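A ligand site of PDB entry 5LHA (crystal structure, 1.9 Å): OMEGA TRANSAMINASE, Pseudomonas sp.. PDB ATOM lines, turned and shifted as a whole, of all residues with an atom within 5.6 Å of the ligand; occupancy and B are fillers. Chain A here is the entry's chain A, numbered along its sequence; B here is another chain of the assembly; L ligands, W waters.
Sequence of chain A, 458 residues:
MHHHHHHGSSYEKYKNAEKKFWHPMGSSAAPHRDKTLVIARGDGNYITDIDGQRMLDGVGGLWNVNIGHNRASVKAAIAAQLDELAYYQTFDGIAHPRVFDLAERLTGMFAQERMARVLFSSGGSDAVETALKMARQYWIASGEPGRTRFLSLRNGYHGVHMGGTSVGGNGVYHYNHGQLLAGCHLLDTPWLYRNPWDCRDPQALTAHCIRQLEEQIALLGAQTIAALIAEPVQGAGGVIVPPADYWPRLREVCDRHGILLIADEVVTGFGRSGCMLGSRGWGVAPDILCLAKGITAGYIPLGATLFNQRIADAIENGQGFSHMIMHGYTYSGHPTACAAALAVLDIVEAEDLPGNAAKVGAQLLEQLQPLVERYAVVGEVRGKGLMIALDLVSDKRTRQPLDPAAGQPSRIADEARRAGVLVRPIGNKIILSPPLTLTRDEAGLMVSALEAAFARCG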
ATOM      1  N   TRP A  63      20.448 -13.789  11.379  1.00  0.00           N
ATOM      2  CA  TRP A  63      20.088 -13.270  10.062  1.00  0.00           C
ATOM      3  C   TRP A  63      18.619 -13.493   9.702  1.00  0.00           C
ATOM      4  O   TRP A  63      18.307 -14.124   8.685  1.00  0.00           O
ATOM      5  CB  TRP A  63      20.951 -13.858   8.935  1.00  0.00           C
ATOM      6  CG  TRP A  63      21.782 -15.104   9.179  1.00  0.00           C
ATOM      7  CD1 TRP A  63      21.456 -16.202   9.935  1.00  0.00           C
ATOM      8  CD2 TRP A  63      23.065 -15.380   8.611  1.00  0.00           C
ATOM      9  NE1 TRP A  63      22.477 -17.125   9.892  1.00  0.00           N
ATOM     10  CE2 TRP A  63      23.476 -16.640   9.082  1.00  0.00           C
ATOM     11  CE3 TRP A  63      23.922 -14.670   7.764  1.00  0.00           C
ATOM     12  CZ2 TRP A  63      24.690 -17.213   8.729  1.00  0.00           C
ATOM     13  CZ3 TRP A  63      25.129 -15.237   7.408  1.00  0.00           C
ATOM     14  CH2 TRP A  63      25.506 -16.491   7.902  1.00  0.00           C
ATOM     15  N   SER A 122       7.605 -24.652  10.025  1.00  0.00           N
ATOM     16  CA  SER A 122       7.850 -23.660  11.071  1.00  0.00           C
ATOM     17  C   SER A 122       9.279 -23.140  11.117  1.00  0.00           C
ATOM     18  O   SER A 122       9.552 -22.221  11.907  1.00  0.00           O
ATOM     19  CB  SER A 122       7.499 -24.238  12.450  1.00  0.00           C
ATOM     20  OG  SER A 122       6.119 -24.562  12.523  1.00  0.00           O
ATOM     21  N   GLY A 123      10.181 -23.656  10.293  1.00  0.00           N
ATOM     22  CA  GLY A 123      11.556 -23.216  10.358  1.00  0.00           C
ATOM     23  C   GLY A 123      12.352 -23.785   9.207  1.00  0.00           C
ATOM     24  O   GLY A 123      11.821 -24.489   8.359  1.00  0.00           O
ATOM     25  N   GLY A 124      13.645 -23.440   9.202  1.00  0.00           N
ATOM     26  CA  GLY A 124      14.506 -23.841   8.100  1.00  0.00           C
ATOM     27  C   GLY A 124      14.843 -25.324   8.083  1.00  0.00           C
ATOM     28  O   GLY A 124      14.896 -25.938   7.024  1.00  0.00           O
ATOM     29  N   SER A 125      15.099 -25.903   9.262  1.00  0.00           N
ATOM     30  CA  SER A 125      15.331 -27.344   9.348  1.00  0.00           C
ATOM     31  C   SER A 125      14.104 -28.126   8.892  1.00  0.00           C
ATOM     32  O   SER A 125      14.238 -29.177   8.263  1.00  0.00           O
ATOM     33  CB  SER A 125      15.697 -27.739  10.769  1.00  0.00           C
ATOM     34  OG  SER A 125      16.879 -27.089  11.183  1.00  0.00           O
ATOM     35  N   ASP A 126      12.906 -27.639   9.250  1.00  0.00           N
ATOM     36  CA  ASP A 126      11.684 -28.230   8.711  1.00  0.00           C
ATOM     37  C   ASP A 126      11.677 -28.188   7.195  1.00  0.00           C
ATOM     38  O   ASP A 126      11.281 -29.163   6.539  1.00  0.00           O
ATOM     39  CB  ASP A 126      10.431 -27.500   9.222  1.00  0.00           C
ATOM     40  CG  ASP A 126      10.284 -27.502  10.703  1.00  0.00           C
ATOM     41  OD1 ASP A 126      11.186 -27.976  11.418  1.00  0.00           O
ATOM     42  OD2 ASP A 126       9.210 -27.044  11.168  1.00  0.00           O
ATOM     43  N   VAL A 128      14.112 -28.004   5.130  1.00  0.00           N
ATOM     44  CA  VAL A 128      15.117 -28.916   4.595  1.00  0.00           C
ATOM     45  C   VAL A 128      14.659 -30.364   4.750  1.00  0.00           C
ATOM     46  O   VAL A 128      14.688 -31.144   3.794  1.00  0.00           O
ATOM     47  CB  VAL A 128      16.478 -28.659   5.261  1.00  0.00           C
ATOM     48  CG1 VAL A 128      17.455 -29.781   4.931  1.00  0.00           C
ATOM     49  CG2 VAL A 128      17.026 -27.291   4.825  1.00  0.00           C
ATOM     50  N   TYR A 157      25.297 -25.934   5.499  1.00  0.00           N
ATOM     51  CA  TYR A 157      24.504 -26.079   6.703  1.00  0.00           C
ATOM     52  C   TYR A 157      23.030 -26.072   6.332  1.00  0.00           C
ATOM     53  O   TYR A 157      22.553 -25.133   5.705  1.00  0.00           O
ATOM     54  CB  TYR A 157      24.830 -24.989   7.724  1.00  0.00           C
ATOM     55  CG  TYR A 157      23.981 -25.106   8.947  1.00  0.00           C
ATOM     56  CD1 TYR A 157      24.203 -26.117   9.890  1.00  0.00           C
ATOM     57  CD2 TYR A 157      22.987 -24.193   9.206  1.00  0.00           C
ATOM     58  CE1 TYR A 157      23.416 -26.217  11.016  1.00  0.00           C
ATOM     59  CE2 TYR A 157      22.208 -24.281  10.334  1.00  0.00           C
ATOM     60  CZ  TYR A 157      22.418 -25.285  11.232  1.00  0.00           C
ATOM     61  OH  TYR A 157      21.637 -25.368  12.343  1.00  0.00           O
ATOM     62  N   HIS A 158      22.308 -27.100   6.795  1.00  0.00           N
ATOM     63  CA  HIS A 158      20.927 -27.307   6.389  1.00  0.00           C
ATOM     64  C   HIS A 158      20.044 -27.682   7.583  1.00  0.00           C
ATOM     65  O   HIS A 158      19.049 -28.403   7.427  1.00  0.00           O
ATOM     66  CB  HIS A 158      20.850 -28.390   5.304  1.00  0.00           C
ATOM     67  CG  HIS A 158      21.797 -28.160   4.174  1.00  0.00           C
ATOM     68  ND1 HIS A 158      21.613 -27.157   3.249  1.00  0.00           N
ATOM     69  CD2 HIS A 158      22.972 -28.766   3.853  1.00  0.00           C
ATOM     70  CE1 HIS A 158      22.623 -27.176   2.378  1.00  0.00           C
ATOM     71  NE2 HIS A 158      23.452 -28.134   2.733  1.00  0.00           N
ATOM     72  N   GLY A 159      20.374 -27.186   8.767  1.00  0.00           N
ATOM     73  CA  GLY A 159      19.567 -27.461   9.950  1.00  0.00           C
ATOM     74  C   GLY A 159      19.983 -28.703  10.719  1.00  0.00           C
ATOM     75  O   GLY A 159      20.968 -29.371  10.399  1.00  0.00           O
ATOM     76  N   VAL A 160      19.176 -29.033  11.726  1.00  0.00           N
ATOM     77  CA  VAL A 160      19.579 -30.029  12.722  1.00  0.00           C
ATOM     78  C   VAL A 160      18.534 -31.106  12.974  1.00  0.00           C
ATOM     79  O   VAL A 160      18.654 -31.863  13.946  1.00  0.00           O
ATOM     80  CB  VAL A 160      19.948 -29.347  14.059  1.00  0.00           C
ATOM     81  CG1 VAL A 160      21.115 -28.400  13.881  1.00  0.00           C
ATOM     82  CG2 VAL A 160      18.756 -28.612  14.613  1.00  0.00           C
ATOM     83  N   GLU A 231      23.428 -24.138  -0.695  1.00  0.00           N
ATOM     84  CA  GLU A 231      23.077 -22.758  -0.379  1.00  0.00           C
ATOM     85  C   GLU A 231      23.670 -21.847  -1.442  1.00  0.00           C
ATOM     86  O   GLU A 231      24.850 -21.985  -1.779  1.00  0.00           O
ATOM     87  CB  GLU A 231      23.615 -22.348   0.979  1.00  0.00           C
ATOM     88  CG  GLU A 231      23.222 -23.234   2.149  1.00  0.00           C
ATOM     89  CD  GLU A 231      24.222 -23.126   3.283  1.00  0.00           C
ATOM     90  OE1 GLU A 231      24.245 -22.099   3.987  1.00  0.00           O
ATOM     91  OE2 GLU A 231      25.034 -24.060   3.449  1.00  0.00           O
ATOM     92  N   ALA A 236      26.286 -20.204   7.547  1.00  0.00           N
ATOM     93  CA  ALA A 236      26.907 -20.606   8.799  1.00  0.00           C
ATOM     94  C   ALA A 236      28.262 -21.257   8.581  1.00  0.00           C
ATOM     95  O   ALA A 236      29.076 -21.281   9.512  1.00  0.00           O
ATOM     96  CB  ALA A 236      25.983 -21.568   9.561  1.00  0.00           C
ATOM     97  N   ASP A 264      18.854 -24.133  -0.875  1.00  0.00           N
ATOM     98  CA  ASP A 264      18.587 -23.786   0.517  1.00  0.00           C
ATOM     99  C   ASP A 264      18.633 -22.270   0.609  1.00  0.00           C
ATOM    100  O   ASP A 264      19.702 -21.669   0.692  1.00  0.00           O
ATOM    101  CB  ASP A 264      19.576 -24.466   1.452  1.00  0.00           C
ATOM    102  CG  ASP A 264      19.233 -24.289   2.914  1.00  0.00           C
ATOM    103  OD1 ASP A 264      18.509 -23.315   3.271  1.00  0.00           O
ATOM    104  OD2 ASP A 264      19.651 -25.152   3.704  1.00  0.00           O
ATOM    105  N   VAL A 266      17.125 -20.489   3.031  1.00  0.00           N
ATOM    106  CA  VAL A 266      16.697 -20.087   4.374  1.00  0.00           C
ATOM    107  C   VAL A 266      17.332 -18.747   4.756  1.00  0.00           C
ATOM    108  O   VAL A 266      16.655 -17.866   5.306  1.00  0.00           O
ATOM    109  CB  VAL A 266      17.012 -21.194   5.391  1.00  0.00           C
ATOM    110  CG1 VAL A 266      16.921 -20.655   6.805  1.00  0.00           C
ATOM    111  CG2 VAL A 266      16.065 -22.374   5.212  1.00  0.00           C
ATOM    112  N   VAL A 267      18.616 -18.571   4.461  1.00  0.00           N
ATOM    113  CA  VAL A 267      19.310 -17.317   4.767  1.00  0.00           C
ATOM    114  C   VAL A 267      19.212 -16.320   3.616  1.00  0.00           C
ATOM    115  O   VAL A 267      18.926 -15.133   3.828  1.00  0.00           O
ATOM    116  CB  VAL A 267      20.776 -17.602   5.162  1.00  0.00           C
ATOM    117  CG1 VAL A 267      21.551 -16.304   5.346  1.00  0.00           C
ATOM    118  CG2 VAL A 267      20.819 -18.403   6.452  1.00  0.00           C
ATOM    119  N   ALA A 292      12.813 -19.851   5.299  1.00  0.00           N
ATOM    120  CA  ALA A 292      12.433 -19.595   6.683  1.00  0.00           C
ATOM    121  C   ALA A 292      12.928 -18.221   7.099  1.00  0.00           C
ATOM    122  O   ALA A 292      13.052 -17.319   6.262  1.00  0.00           O
ATOM    123  CB  ALA A 292      12.989 -20.662   7.623  1.00  0.00           C
ATOM    124  N   LYS A 293      13.251 -18.059   8.381  1.00  0.00           N
ATOM    125  CA  LYS A 293      13.889 -16.863   8.923  1.00  0.00           C
ATOM    126  C   LYS A 293      13.185 -15.569   8.524  1.00  0.00           C
ATOM    127  O   LYS A 293      12.110 -15.239   9.045  1.00  0.00           O
ATOM    128  CB  LYS A 293      15.355 -16.816   8.488  1.00  0.00           C
ATOM    129  CG  LYS A 293      16.237 -17.830   9.201  1.00  0.00           C
ATOM    130  CD  LYS A 293      17.687 -17.632   8.849  1.00  0.00           C
ATOM    131  CE  LYS A 293      18.576 -18.647   9.550  1.00  0.00           C
ATOM    132  NZ  LYS A 293      18.720 -18.348  11.005  1.00  0.00           N
ATOM    133  N   PHE B  91      21.114 -18.534  21.070  1.00  0.00           N
ATOM    134  CA  PHE B  91      22.325 -19.291  20.808  1.00  0.00           C
ATOM    135  C   PHE B  91      23.421 -18.885  21.801  1.00  0.00           C
ATOM    136  O   PHE B  91      23.309 -17.879  22.506  1.00  0.00           O
ATOM    137  CB  PHE B  91      22.769 -19.088  19.358  1.00  0.00           C
ATOM    138  CG  PHE B  91      21.964 -19.898  18.358  1.00  0.00           C
ATOM    139  CD1 PHE B  91      20.645 -20.239  18.624  1.00  0.00           C
ATOM    140  CD2 PHE B  91      22.534 -20.325  17.169  1.00  0.00           C
ATOM    141  CE1 PHE B  91      19.911 -20.970  17.722  1.00  0.00           C
ATOM    142  CE2 PHE B  91      21.807 -21.067  16.263  1.00  0.00           C
ATOM    143  CZ  PHE B  91      20.488 -21.402  16.537  1.00  0.00           C
ATOM    144  N   GLY B 328      19.811 -27.386  17.814  1.00  0.00           N
ATOM    145  CA  GLY B 328      18.845 -26.360  18.172  1.00  0.00           C
ATOM    146  C   GLY B 328      18.448 -25.549  16.965  1.00  0.00           C
ATOM    147  O   GLY B 328      18.942 -25.745  15.849  1.00  0.00           O
ATOM    148  N   TYR B 329      17.552 -24.594  17.220  1.00  0.00           N
ATOM    149  CA  TYR B 329      16.788 -23.941  16.173  1.00  0.00           C
ATOM    150  C   TYR B 329      16.823 -22.428  16.308  1.00  0.00           C
ATOM    151  O   TYR B 329      16.968 -21.891  17.418  1.00  0.00           O
ATOM    152  CB  TYR B 329      15.343 -24.456  16.190  1.00  0.00           C
ATOM    153  CG  TYR B 329      15.284 -25.959  16.114  1.00  0.00           C
ATOM    154  CD1 TYR B 329      15.510 -26.621  14.913  1.00  0.00           C
ATOM    155  CD2 TYR B 329      15.051 -26.727  17.265  1.00  0.00           C
ATOM    156  CE1 TYR B 329      15.478 -28.008  14.841  1.00  0.00           C
ATOM    157  CE2 TYR B 329      15.027 -28.118  17.197  1.00  0.00           C
ATOM    158  CZ  TYR B 329      15.243 -28.747  15.982  1.00  0.00           C
ATOM    159  OH  TYR B 329      15.202 -30.130  15.881  1.00  0.00           O
ATOM    160  N   THR B 330      16.703 -21.744  15.162  1.00  0.00           N
ATOM    161  CA  THR B 330      16.568 -20.295  15.128  1.00  0.00           C
ATOM    162  C   THR B 330      15.533 -19.820  16.127  1.00  0.00           C
ATOM    163  O   THR B 330      15.732 -18.802  16.813  1.00  0.00           O
ATOM    164  CB  THR B 330      16.145 -19.844  13.716  1.00  0.00           C
ATOM    165  OG1 THR B 330      17.140 -20.222  12.770  1.00  0.00           O
ATOM    166  CG2 THR B 330      15.935 -18.336  13.650  1.00  0.00           C
ATOM    167  N   TYR B 331      14.428 -20.551  16.248  1.00  0.00           N
ATOM    168  CA  TYR B 331      13.301 -20.145  17.076  1.00  0.00           C
ATOM    169  C   TYR B 331      13.246 -20.905  18.404  1.00  0.00           C
ATOM    170  O   TYR B 331      12.204 -20.875  19.072  1.00  0.00           O
ATOM    171  CB  TYR B 331      12.005 -20.313  16.277  1.00  0.00           C
ATOM    172  CG  TYR B 331      11.986 -19.450  15.025  1.00  0.00           C
ATOM    173  CD1 TYR B 331      12.414 -18.126  15.068  1.00  0.00           C
ATOM    174  CD2 TYR B 331      11.568 -19.968  13.802  1.00  0.00           C
ATOM    175  CE1 TYR B 331      12.414 -17.340  13.932  1.00  0.00           C
ATOM    176  CE2 TYR B 331      11.573 -19.189  12.645  1.00  0.00           C
ATOM    177  CZ  TYR B 331      11.990 -17.874  12.723  1.00  0.00           C
ATOM    178  OH  TYR B 331      11.999 -17.104  11.599  1.00  0.00           O
HETATM  179  N1  LIG L   1      19.623 -24.011   6.348  1.00  0.00           N
HETATM  180  C1  LIG L   1      20.231 -22.762   6.402  1.00  0.00           C
HETATM  181  C2  LIG L   1      21.028 -22.243   5.236  1.00  0.00           C
HETATM  182  C3  LIG L   1      20.415 -22.185   7.645  1.00  0.00           C
HETATM  183  O1  LIG L   1      21.313 -21.164   7.805  1.00  0.00           O
HETATM  184  C4  LIG L   1      19.689 -22.657   8.739  1.00  0.00           C
HETATM  185  C5  LIG L   1      19.838 -21.961  10.082  1.00  0.00           C
HETATM  186  N2  LIG L   1      20.888 -20.972  10.034  1.00  0.00           N
HETATM  187  C6  LIG L   1      18.852 -23.761   8.606  1.00  0.00           C
HETATM  188  C7  LIG L   1      18.827 -24.437   7.382  1.00  0.00           C
HETATM  189  C8  LIG L   1      17.982 -24.195   9.771  1.00  0.00           C
HETATM  190  O2  LIG L   1      17.089 -23.160  10.154  1.00  0.00           O
HETATM  191  P1  LIG L   1      16.267 -23.192  11.540  1.00  0.00           P
HETATM  192  O3  LIG L   1      17.198 -22.656  12.619  1.00  0.00           O
HETATM  193  O4  LIG L   1      15.075 -22.265  11.408  1.00  0.00           O
HETATM  194  O5  LIG L   1      15.807 -24.585  11.925  1.00  0.00           O
HETATM  195  O   HOH W   1      14.357 -19.999  10.713  1.00  0.00           O
HETATM  196  O   HOH W   2      22.056 -19.471  11.906  1.00  0.00           O
HETATM  197  O   HOH W   3      13.747 -22.092  14.021  1.00  0.00           O
HETATM  198  O   HOH W   4      24.115 -21.097   6.664  1.00  0.00           O
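N of Thr 330 of chain B is in hydrogen-bond range of O3 of the ligand. An oxygen (O5) of the ligand is in hydrogen-bond range of the backbone NH (N) of Ser 125 (3.1 Å). OG1 of Thr 330 of chain B sits at hydrogen-bond distance from O3 of the ligand. N of Gly 124 sits at hydrogen-bond distance from O4 of the ligand (2.9 Å). The side-chain hydroxyl of Ser 125 is in hydrogen-bond range of an oxygen (O5) of the ligand (2.8 Å). The side-chain carboxylate (OD2) of Asp 264 is in hydrogen-bond range of a nitrogen (N1) of the ligand (2.9 Å).
OG1 of Thr 330 of chain B lies within hydrogen-bond range of NZ of Lys 293, at 3.0 Å. The side-chain hydroxyl of Ser 125 is in hydrogen-bond range of the backbone NH of Val 160 (3.1 Å). OD1 of Asp 264 sits at hydrogen-bond distance from N of Val 266 (3.2 Å). The side-chain carboxylate of Glu 231 is in hydrogen-bond range of the backbone NH of Tyr 157 (2.8 Å). A ring nitrogen (ND1) of His 158 is in hydrogen-bond range of the side-chain carboxylate of Asp 264, at 2.8 Å. The side-chain hydroxyl (OH) of Tyr 331 of chain B lies within hydrogen-bond range of the backbone carbonyl oxygen (O) of Lys 293, 3.2 Å away.
The backbone carbonyl oxygen (O) of Tyr 157 sits close to a nitrogen (N1) of the ligand. Gly 123 touches the ligand (CA to O4, 3.8 Å). His 158 touches the ligand. Gly 159 touches the ligand. Glu 231 touches the ligand (OE1 to C2, 3.5 Å). Val 266 touches the ligand. Val 267 touches the ligand (CG2 to O1, 3.1 Å). Lys 293 touches the ligand (CE to N2, 3.3 Å). CD1 of Tyr 329 of chain B touches O5 of the ligand, at 3.6 Å. Hydrophobic or aromatic side chains that line the ligand: Tyr 157, Val 266, Val 267 and Tyr 329 of chain B. 13 residues have an atom within 4 Å of the ligand: Gly 123, Gly 124, Ser 125, Tyr 157, His 158, Gly 159, Glu 231, Asp 264, Val 266, Val 267, Lys 293, Tyr 329 of chain B and Thr 330 of chain B.
Water W1 lies within hydrogen-bond range of O4 of the ligand (2.5 Å), N of Lys 293 (3.2 Å) and OG1 of Thr 330 of chain B (3.5 Å). Water W2 bridges a nitrogen (N2) of the ligand (2.7 Å) and the indole nitrogen (NE1) of Trp 63 (3.1 Å). Water W3 lies within hydrogen-bond range of N of Tyr 331 of chain B (2.8 Å), O4 of the ligand (2.9 Å) and N of Thr 330 of chain B (3.2 Å). Water W4 lies within hydrogen-bond range of the backbone NH of Ala 236 (2.5 Å), the side-chain carboxylate of Glu 231 (2.9 Å) and an oxygen (O1) of the ligand (3.0 Å).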
